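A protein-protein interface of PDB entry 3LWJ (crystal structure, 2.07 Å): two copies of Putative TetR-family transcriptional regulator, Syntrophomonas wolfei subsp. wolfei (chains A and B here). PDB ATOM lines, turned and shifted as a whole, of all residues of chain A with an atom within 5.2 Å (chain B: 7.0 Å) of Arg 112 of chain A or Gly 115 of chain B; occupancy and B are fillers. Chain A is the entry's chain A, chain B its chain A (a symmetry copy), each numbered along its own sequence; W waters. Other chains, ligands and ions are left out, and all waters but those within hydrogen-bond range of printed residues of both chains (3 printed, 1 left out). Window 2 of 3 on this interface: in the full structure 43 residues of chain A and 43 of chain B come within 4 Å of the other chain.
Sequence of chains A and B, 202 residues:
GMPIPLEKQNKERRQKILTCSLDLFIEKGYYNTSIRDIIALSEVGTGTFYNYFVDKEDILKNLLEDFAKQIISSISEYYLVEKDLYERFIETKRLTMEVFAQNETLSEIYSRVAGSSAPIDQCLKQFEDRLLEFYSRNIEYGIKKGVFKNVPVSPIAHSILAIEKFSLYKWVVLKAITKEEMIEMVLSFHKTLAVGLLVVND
Arg 112 of chain A touches Ala 114 of chain B, and with the chains exchanged Ala 114 of chain A touches Arg 112 of chain B.
Water W2 lies within hydrogen-bond range of OH of Tyr 169 of chain A (2.5 Å) and O of Asp 121 of chain B (2.8 Å). Water W1 lies within hydrogen-bond range of the backbone carbonyl oxygen of Ala 114 of chain A, the backbone NH of Ala 114 of chain B and the backbone carbonyl oxygen of Arg 112 of chain B. Water W3 lies within hydrogen-bond range of O of Val 173 of chain A and OD2 of Asp 121 of chain B.
Arg 112 of chain A touches just these residues of chain B: Ala 114 and Gly 115. Of the printed residues of chain A, Gly 115 of chain B touches Ser 111, Arg 112 and Tyr 169. Of the printed residues of chain B, Tyr 169 of chain A touches Gly 115 and Asp 121. Of the printed residues of chain A, Asp 121 of chain B touches Tyr 169 (2.6 Å) and Val 173 (3.7 Å). Of the printed residues of chain B, Ala 114 of chain A touches Arg 112. Of the printed residues of chain B, Val 173 of chain A touches Asp 121 (3.7 Å). The nearest residue of chain B that does not touch Arg 112 of chain A is Asp 121 of chain B (4.3 Å). The nearest printed residue of chain B that does not touch Val 173 of chain A is Gly 115 of chain B (4.2 Å).
The backbone NH (N) of Gly 115 of chain B is in hydrogen-bond range of the side-chain carboxylate (OD1) of Asp 121 of chain B. The backbone carbonyl oxygen of Ser 107 of chain A sits at hydrogen-bond distance from the side-chain hydroxyl of Ser 111 of chain A (2.7 Å). The side-chain carboxylate (OE2) of Glu 108 of chain A lies within salt-bridge range of the guanidinium group (NE) of Arg 112 of chain A, at 3.0 Å.
Among the printed residues, pairs that only touch across the chains: Tyr 169 of chain A with Gly 115 of chain B (3.6 Å), Val 173 of chain A with Asp 121 of chain B (3.7 Å), Arg 112 of chain A with Ala 114 of chain B (3.7 Å), Ala 114 of chain A with Arg 112 of chain B (3.8 Å) and Ser 111 of chain A with Gly 115 of chain B (3.98 Å).
The guanidinium group (NH1) of Arg 112 of chain A lies within hydrogen-bond range of the backbone carbonyl oxygen (O) of Gly 115 of chain B (2.9 Å). OH of Tyr 169 of chain A sits at hydrogen-bond distance from OD1 of Asp 121 of chain B (2.6 Å).
Of the 11 printed residues of chain B, 4 touch a printed residue of chain A. Printed residues of chain A that touch a printed residue of chain B: Ser 111, Arg 112, Ala 114, Tyr 169 and Val 173. Hydrophobic or aromatic side chains of chain A within 4 Å of the printed part of chain B: Tyr 169 and Val 173.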
ATOM      1  N   SER A 107      18.683  -5.332   8.048  1.00  0.00           N
ATOM      2  CA  SER A 107      19.828  -4.786   8.779  1.00  0.00           C
ATOM      3  C   SER A 107      20.952  -4.473   7.800  1.00  0.00           C
ATOM      4  O   SER A 107      21.606  -3.448   7.891  1.00  0.00           O
ATOM      5  CB  SER A 107      20.321  -5.775   9.857  1.00  0.00           C
ATOM      6  OG  SER A 107      19.405  -5.888  10.973  1.00  0.00           O
ATOM      7  N   GLU A 108      21.177  -5.351   6.840  1.00  0.00           N
ATOM      8  CA  GLU A 108      22.168  -5.064   5.809  1.00  0.00           C
ATOM      9  C   GLU A 108      21.824  -3.802   5.001  1.00  0.00           C
ATOM     10  O   GLU A 108      22.666  -2.911   4.875  1.00  0.00           O
ATOM     11  CB  GLU A 108      22.354  -6.244   4.878  1.00  0.00           C
ATOM     12  CG  GLU A 108      23.753  -6.274   4.277  1.00  0.00           C
ATOM     13  CD  GLU A 108      23.947  -7.391   3.250  1.00  0.00           C
ATOM     14  OE1 GLU A 108      23.540  -8.548   3.517  1.00  0.00           O
ATOM     15  OE2 GLU A 108      24.498  -7.077   2.171  1.00  0.00           O
ATOM     16  N   ILE A 109      20.598  -3.718   4.460  1.00  0.00           N
ATOM     17  CA  ILE A 109      20.198  -2.541   3.694  1.00  0.00           C
ATOM     18  C   ILE A 109      20.339  -1.280   4.552  1.00  0.00           C
ATOM     19  O   ILE A 109      20.952  -0.328   4.118  1.00  0.00           O
ATOM     20  CB  ILE A 109      18.750  -2.627   3.176  1.00  0.00           C
ATOM     21  CG1 ILE A 109      18.582  -3.748   2.146  1.00  0.00           C
ATOM     22  CG2 ILE A 109      18.282  -1.266   2.564  1.00  0.00           C
ATOM     23  CD1 ILE A 109      19.479  -3.634   0.939  1.00  0.00           C
ATOM     24  N   TYR A 110      19.802  -1.302   5.780  1.00  0.00           N
ATOM     25  CA  TYR A 110      19.969  -0.191   6.742  1.00  0.00           C
ATOM     26  C   TYR A 110      21.414   0.238   6.904  1.00  0.00           C
ATOM     27  O   TYR A 110      21.705   1.438   7.003  1.00  0.00           O
ATOM     28  CB  TYR A 110      19.377  -0.616   8.076  1.00  0.00           C
ATOM     29  CG  TYR A 110      19.625   0.272   9.261  1.00  0.00           C
ATOM     30  CD1 TYR A 110      19.296   1.640   9.237  1.00  0.00           C
ATOM     31  CD2 TYR A 110      20.127  -0.274  10.455  1.00  0.00           C
ATOM     32  CE1 TYR A 110      19.509   2.446  10.374  1.00  0.00           C
ATOM     33  CE2 TYR A 110      20.327   0.525  11.588  1.00  0.00           C
ATOM     34  CZ  TYR A 110      20.001   1.882  11.531  1.00  0.00           C
ATOM     35  OH  TYR A 110      20.203   2.661  12.637  1.00  0.00           O
ATOM     36  N   SER A 111      22.312  -0.746   6.935  1.00  0.00           N
ATOM     37  CA  SER A 111      23.742  -0.528   7.183  1.00  0.00           C
ATOM     38  C   SER A 111      24.501  -0.114   5.949  1.00  0.00           C
ATOM     39  O   SER A 111      25.660   0.280   6.046  1.00  0.00           O
ATOM     40  CB  SER A 111      24.395  -1.812   7.727  1.00  0.00           C
ATOM     41  OG  SER A 111      23.795  -2.215   8.945  1.00  0.00           O
ATOM     42  N   ARG A 112      23.873  -0.227   4.793  1.00  0.00           N
ATOM     43  CA  ARG A 112      24.535   0.115   3.536  1.00  0.00           C
ATOM     44  C   ARG A 112      24.076   1.452   2.933  1.00  0.00           C
ATOM     45  O   ARG A 112      24.866   2.119   2.302  1.00  0.00           O
ATOM     46  CB  ARG A 112      24.328  -0.989   2.507  1.00  0.00           C
ATOM     47  CG  ARG A 112      25.084  -2.271   2.815  1.00  0.00           C
ATOM     48  CD  ARG A 112      24.992  -3.235   1.624  1.00  0.00           C
ATOM     49  NE  ARG A 112      25.877  -4.386   1.817  1.00  0.00           N
ATOM     50  CZ  ARG A 112      27.195  -4.352   1.643  1.00  0.00           C
ATOM     51  NH1 ARG A 112      27.797  -3.222   1.266  1.00  0.00           N
ATOM     52  NH2 ARG A 112      27.922  -5.447   1.855  1.00  0.00           N
ATOM     53  N   VAL A 113      22.814   1.829   3.122  1.00  0.00           N
ATOM     54  CA  VAL A 113      22.282   2.987   2.412  1.00  0.00           C
ATOM     55  C   VAL A 113      22.361   4.322   3.178  1.00  0.00           C
ATOM     56  O   VAL A 113      22.027   5.361   2.615  1.00  0.00           O
ATOM     57  CB  VAL A 113      20.836   2.754   1.933  1.00  0.00           C
ATOM     58  CG1 VAL A 113      20.750   1.469   1.054  1.00  0.00           C
ATOM     59  CG2 VAL A 113      19.850   2.790   3.108  1.00  0.00           C
ATOM     60  N   ALA A 114      22.802   4.299   4.435  1.00  0.00           N
ATOM     61  CA  ALA A 114      22.995   5.533   5.224  1.00  0.00           C
ATOM     62  C   ALA A 114      23.939   6.506   4.548  1.00  0.00           C
ATOM     63  O   ALA A 114      24.998   6.097   4.098  1.00  0.00           O
ATOM     64  CB  ALA A 114      23.505   5.187   6.620  1.00  0.00           C
ATOM     65  N   TYR A 169      26.882  -2.835  11.522  1.00  0.00           N
ATOM     66  CA  TYR A 169      27.584  -2.662  10.259  1.00  0.00           C
ATOM     67  C   TYR A 169      28.831  -3.553  10.182  1.00  0.00           C
ATOM     68  O   TYR A 169      29.075  -4.199   9.168  1.00  0.00           O
ATOM     69  CB  TYR A 169      27.918  -1.182  10.049  1.00  0.00           C
ATOM     70  CG  TYR A 169      29.098  -0.857   9.152  1.00  0.00           C
ATOM     71  CD1 TYR A 169      28.950  -0.702   7.785  1.00  0.00           C
ATOM     72  CD2 TYR A 169      30.359  -0.643   9.693  1.00  0.00           C
ATOM     73  CE1 TYR A 169      30.052  -0.363   6.976  1.00  0.00           C
ATOM     74  CE2 TYR A 169      31.456  -0.282   8.896  1.00  0.00           C
ATOM     75  CZ  TYR A 169      31.298  -0.157   7.539  1.00  0.00           C
ATOM     76  OH  TYR A 169      32.395   0.210   6.756  1.00  0.00           O
ATOM     77  N   VAL A 172      27.307  -7.406   9.820  1.00  0.00           N
ATOM     78  CA  VAL A 172      26.560  -7.749   8.622  1.00  0.00           C
ATOM     79  C   VAL A 172      27.166  -7.188   7.330  1.00  0.00           C
ATOM     80  O   VAL A 172      26.992  -7.794   6.285  1.00  0.00           O
ATOM     81  CB  VAL A 172      25.021  -7.385   8.750  1.00  0.00           C
ATOM     82  CG1 VAL A 172      24.760  -5.866   8.544  1.00  0.00           C
ATOM     83  CG2 VAL A 172      24.213  -8.210   7.787  1.00  0.00           C
ATOM     84  N   VAL A 173      27.858  -6.052   7.372  1.00  0.00           N
ATOM     85  CA  VAL A 173      28.485  -5.541   6.159  1.00  0.00           C
ATOM     86  C   VAL A 173      29.979  -5.911   6.066  1.00  0.00           C
ATOM     87  O   VAL A 173      30.383  -6.534   5.081  1.00  0.00           O
ATOM     88  CB  VAL A 173      28.291  -4.047   5.952  1.00  0.00           C
ATOM     89  CG1 VAL A 173      29.109  -3.555   4.768  1.00  0.00           C
ATOM     90  CG2 VAL A 173      26.796  -3.730   5.752  1.00  0.00           C
ATOM     91  N   TYR B  31      31.484   7.499  -6.784  1.00  0.00           N
ATOM     92  CA  TYR B  31      31.394   6.434  -7.791  1.00  0.00           C
ATOM     93  C   TYR B  31      31.299   6.944  -9.220  1.00  0.00           C
ATOM     94  O   TYR B  31      31.874   6.320 -10.153  1.00  0.00           O
ATOM     95  CB  TYR B  31      30.231   5.501  -7.465  1.00  0.00           C
ATOM     96  CG  TYR B  31      30.567   4.680  -6.247  1.00  0.00           C
ATOM     97  CD1 TYR B  31      31.550   3.683  -6.319  1.00  0.00           C
ATOM     98  CD2 TYR B  31      29.974   4.934  -5.028  1.00  0.00           C
ATOM     99  CE1 TYR B  31      31.884   2.929  -5.230  1.00  0.00           C
ATOM    100  CE2 TYR B  31      30.316   4.201  -3.904  1.00  0.00           C
ATOM    101  CZ  TYR B  31      31.272   3.191  -4.009  1.00  0.00           C
ATOM    102  OH  TYR B  31      31.612   2.445  -2.906  1.00  0.00           O
ATOM    103  N   ARG B 112      29.312   9.592   3.902  1.00  0.00           N
ATOM    104  CA  ARG B 112      28.389   9.185   2.845  1.00  0.00           C
ATOM    105  C   ARG B 112      28.711   7.813   2.231  1.00  0.00           C
ATOM    106  O   ARG B 112      27.805   7.117   1.829  1.00  0.00           O
ATOM    107  CB  ARG B 112      28.355  10.228   1.737  1.00  0.00           C
ATOM    108  CG  ARG B 112      27.678  11.530   2.133  1.00  0.00           C
ATOM    109  CD  ARG B 112      27.497  12.426   0.899  1.00  0.00           C
ATOM    110  NE  ARG B 112      26.670  13.591   1.220  1.00  0.00           N
ATOM    111  CZ  ARG B 112      25.346  13.555   1.345  1.00  0.00           C
ATOM    112  NH1 ARG B 112      24.682  12.410   1.175  1.00  0.00           N
ATOM    113  NH2 ARG B 112      24.678  14.665   1.653  1.00  0.00           N
ATOM    114  N   VAL B 113      29.986   7.440   2.155  1.00  0.00           N
ATOM    115  CA  VAL B 113      30.353   6.240   1.409  1.00  0.00           C
ATOM    116  C   VAL B 113      30.455   4.950   2.248  1.00  0.00           C
ATOM    117  O   VAL B 113      30.661   3.880   1.683  1.00  0.00           O
ATOM    118  CB  VAL B 113      31.655   6.437   0.609  1.00  0.00           C
ATOM    119  CG1 VAL B 113      31.535   7.671  -0.338  1.00  0.00           C
ATOM    120  CG2 VAL B 113      32.878   6.461   1.535  1.00  0.00           C
ATOM    121  N   ALA B 114      30.305   5.047   3.568  1.00  0.00           N
ATOM    122  CA  ALA B 114      30.300   3.860   4.448  1.00  0.00           C
ATOM    123  C   ALA B 114      29.235   2.857   4.054  1.00  0.00           C
ATOM    124  O   ALA B 114      28.100   3.246   3.829  1.00  0.00           O
ATOM    125  CB  ALA B 114      30.111   4.286   5.901  1.00  0.00           C
ATOM    126  N   GLY B 115      29.615   1.571   3.933  1.00  0.00           N
ATOM    127  CA  GLY B 115      28.715   0.481   3.501  1.00  0.00           C
ATOM    128  C   GLY B 115      28.370   0.407   2.032  1.00  0.00           C
ATOM    129  O   GLY B 115      27.507  -0.385   1.629  1.00  0.00           O
ATOM    130  N   SER B 116      29.029   1.230   1.215  1.00  0.00           N
ATOM    131  CA  SER B 116      28.683   1.359  -0.208  1.00  0.00           C
ATOM    132  C   SER B 116      29.207   0.184  -1.054  1.00  0.00           C
ATOM    133  O   SER B 116      28.518  -0.284  -1.959  1.00  0.00           O
ATOM    134  CB  SER B 116      29.189   2.706  -0.761  1.00  0.00           C
ATOM    135  OG  SER B 116      30.617   2.824  -0.726  1.00  0.00           O
ATOM    136  N   SER B 117      30.435  -0.272  -0.799  1.00  0.00           N
ATOM    137  CA  SER B 117      30.987  -1.446  -1.510  1.00  0.00           C
ATOM    138  C   SER B 117      32.153  -1.969  -0.732  1.00  0.00           C
ATOM    139  O   SER B 117      32.699  -1.240   0.084  1.00  0.00           O
ATOM    140  CB  SER B 117      31.458  -1.076  -2.916  1.00  0.00           C
ATOM    141  OG  SER B 117      32.657  -0.322  -2.899  1.00  0.00           O
ATOM    142  N   ALA B 118      32.562  -3.217  -0.983  1.00  0.00           N
ATOM    143  CA  ALA B 118      33.626  -3.822  -0.171  1.00  0.00           C
ATOM    144  C   ALA B 118      34.980  -3.131  -0.345  1.00  0.00           C
ATOM    145  O   ALA B 118      35.703  -2.962   0.630  1.00  0.00           O
ATOM    146  CB  ALA B 118      33.755  -5.316  -0.411  1.00  0.00           C
ATOM    147  N   ILE B 120      35.599   0.036  -0.845  1.00  0.00           N
ATOM    148  CA  ILE B 120      35.559   1.341  -0.138  1.00  0.00           C
ATOM    149  C   ILE B 120      35.449   1.090   1.359  1.00  0.00           C
ATOM    150  O   ILE B 120      36.160   1.719   2.153  1.00  0.00           O
ATOM    151  CB  ILE B 120      34.450   2.230  -0.701  1.00  0.00           C
ATOM    152  CG1 ILE B 120      34.937   2.855  -2.022  1.00  0.00           C
ATOM    153  CG2 ILE B 120      34.071   3.340   0.283  1.00  0.00           C
ATOM    154  CD1 ILE B 120      35.223   1.883  -3.167  1.00  0.00           C
ATOM    155  N   ASP B 121      34.628   0.110   1.742  1.00  0.00           N
ATOM    156  CA  ASP B 121      34.601  -0.320   3.148  1.00  0.00           C
ATOM    157  C   ASP B 121      35.964  -0.826   3.654  1.00  0.00           C
ATOM    158  O   ASP B 121      36.350  -0.526   4.789  1.00  0.00           O
ATOM    159  CB  ASP B 121      33.485  -1.320   3.385  1.00  0.00           C
ATOM    160  CG  ASP B 121      32.122  -0.644   3.483  1.00  0.00           C
ATOM    161  OD1 ASP B 121      32.010   0.399   4.188  1.00  0.00           O
ATOM    162  OD2 ASP B 121      31.160  -1.171   2.887  1.00  0.00           O
ATOM    163  N   LEU B 124      37.797   2.356   4.475  1.00  0.00           N
ATOM    164  CA  LEU B 124      37.332   2.981   5.708  1.00  0.00           C
ATOM    165  C   LEU B 124      37.787   2.133   6.883  1.00  0.00           C
ATOM    166  O   LEU B 124      38.041   2.673   7.930  1.00  0.00           O
ATOM    167  CB  LEU B 124      35.821   3.218   5.711  1.00  0.00           C
ATOM    168  CG  LEU B 124      35.402   4.606   5.180  1.00  0.00           C
ATOM    169  CD1 LEU B 124      35.782   4.823   3.683  1.00  0.00           C
ATOM    170  CD2 LEU B 124      33.920   4.822   5.377  1.00  0.00           C
HETATM  171  O   HOH W   1      27.832   6.348   4.945  1.00  0.00           O
HETATM  172  O   HOH W   2      34.854  -0.126   7.160  1.00  0.00           O
HETATM  173  O   HOH W   3      31.858  -4.557   2.796  1.00  0.00           O
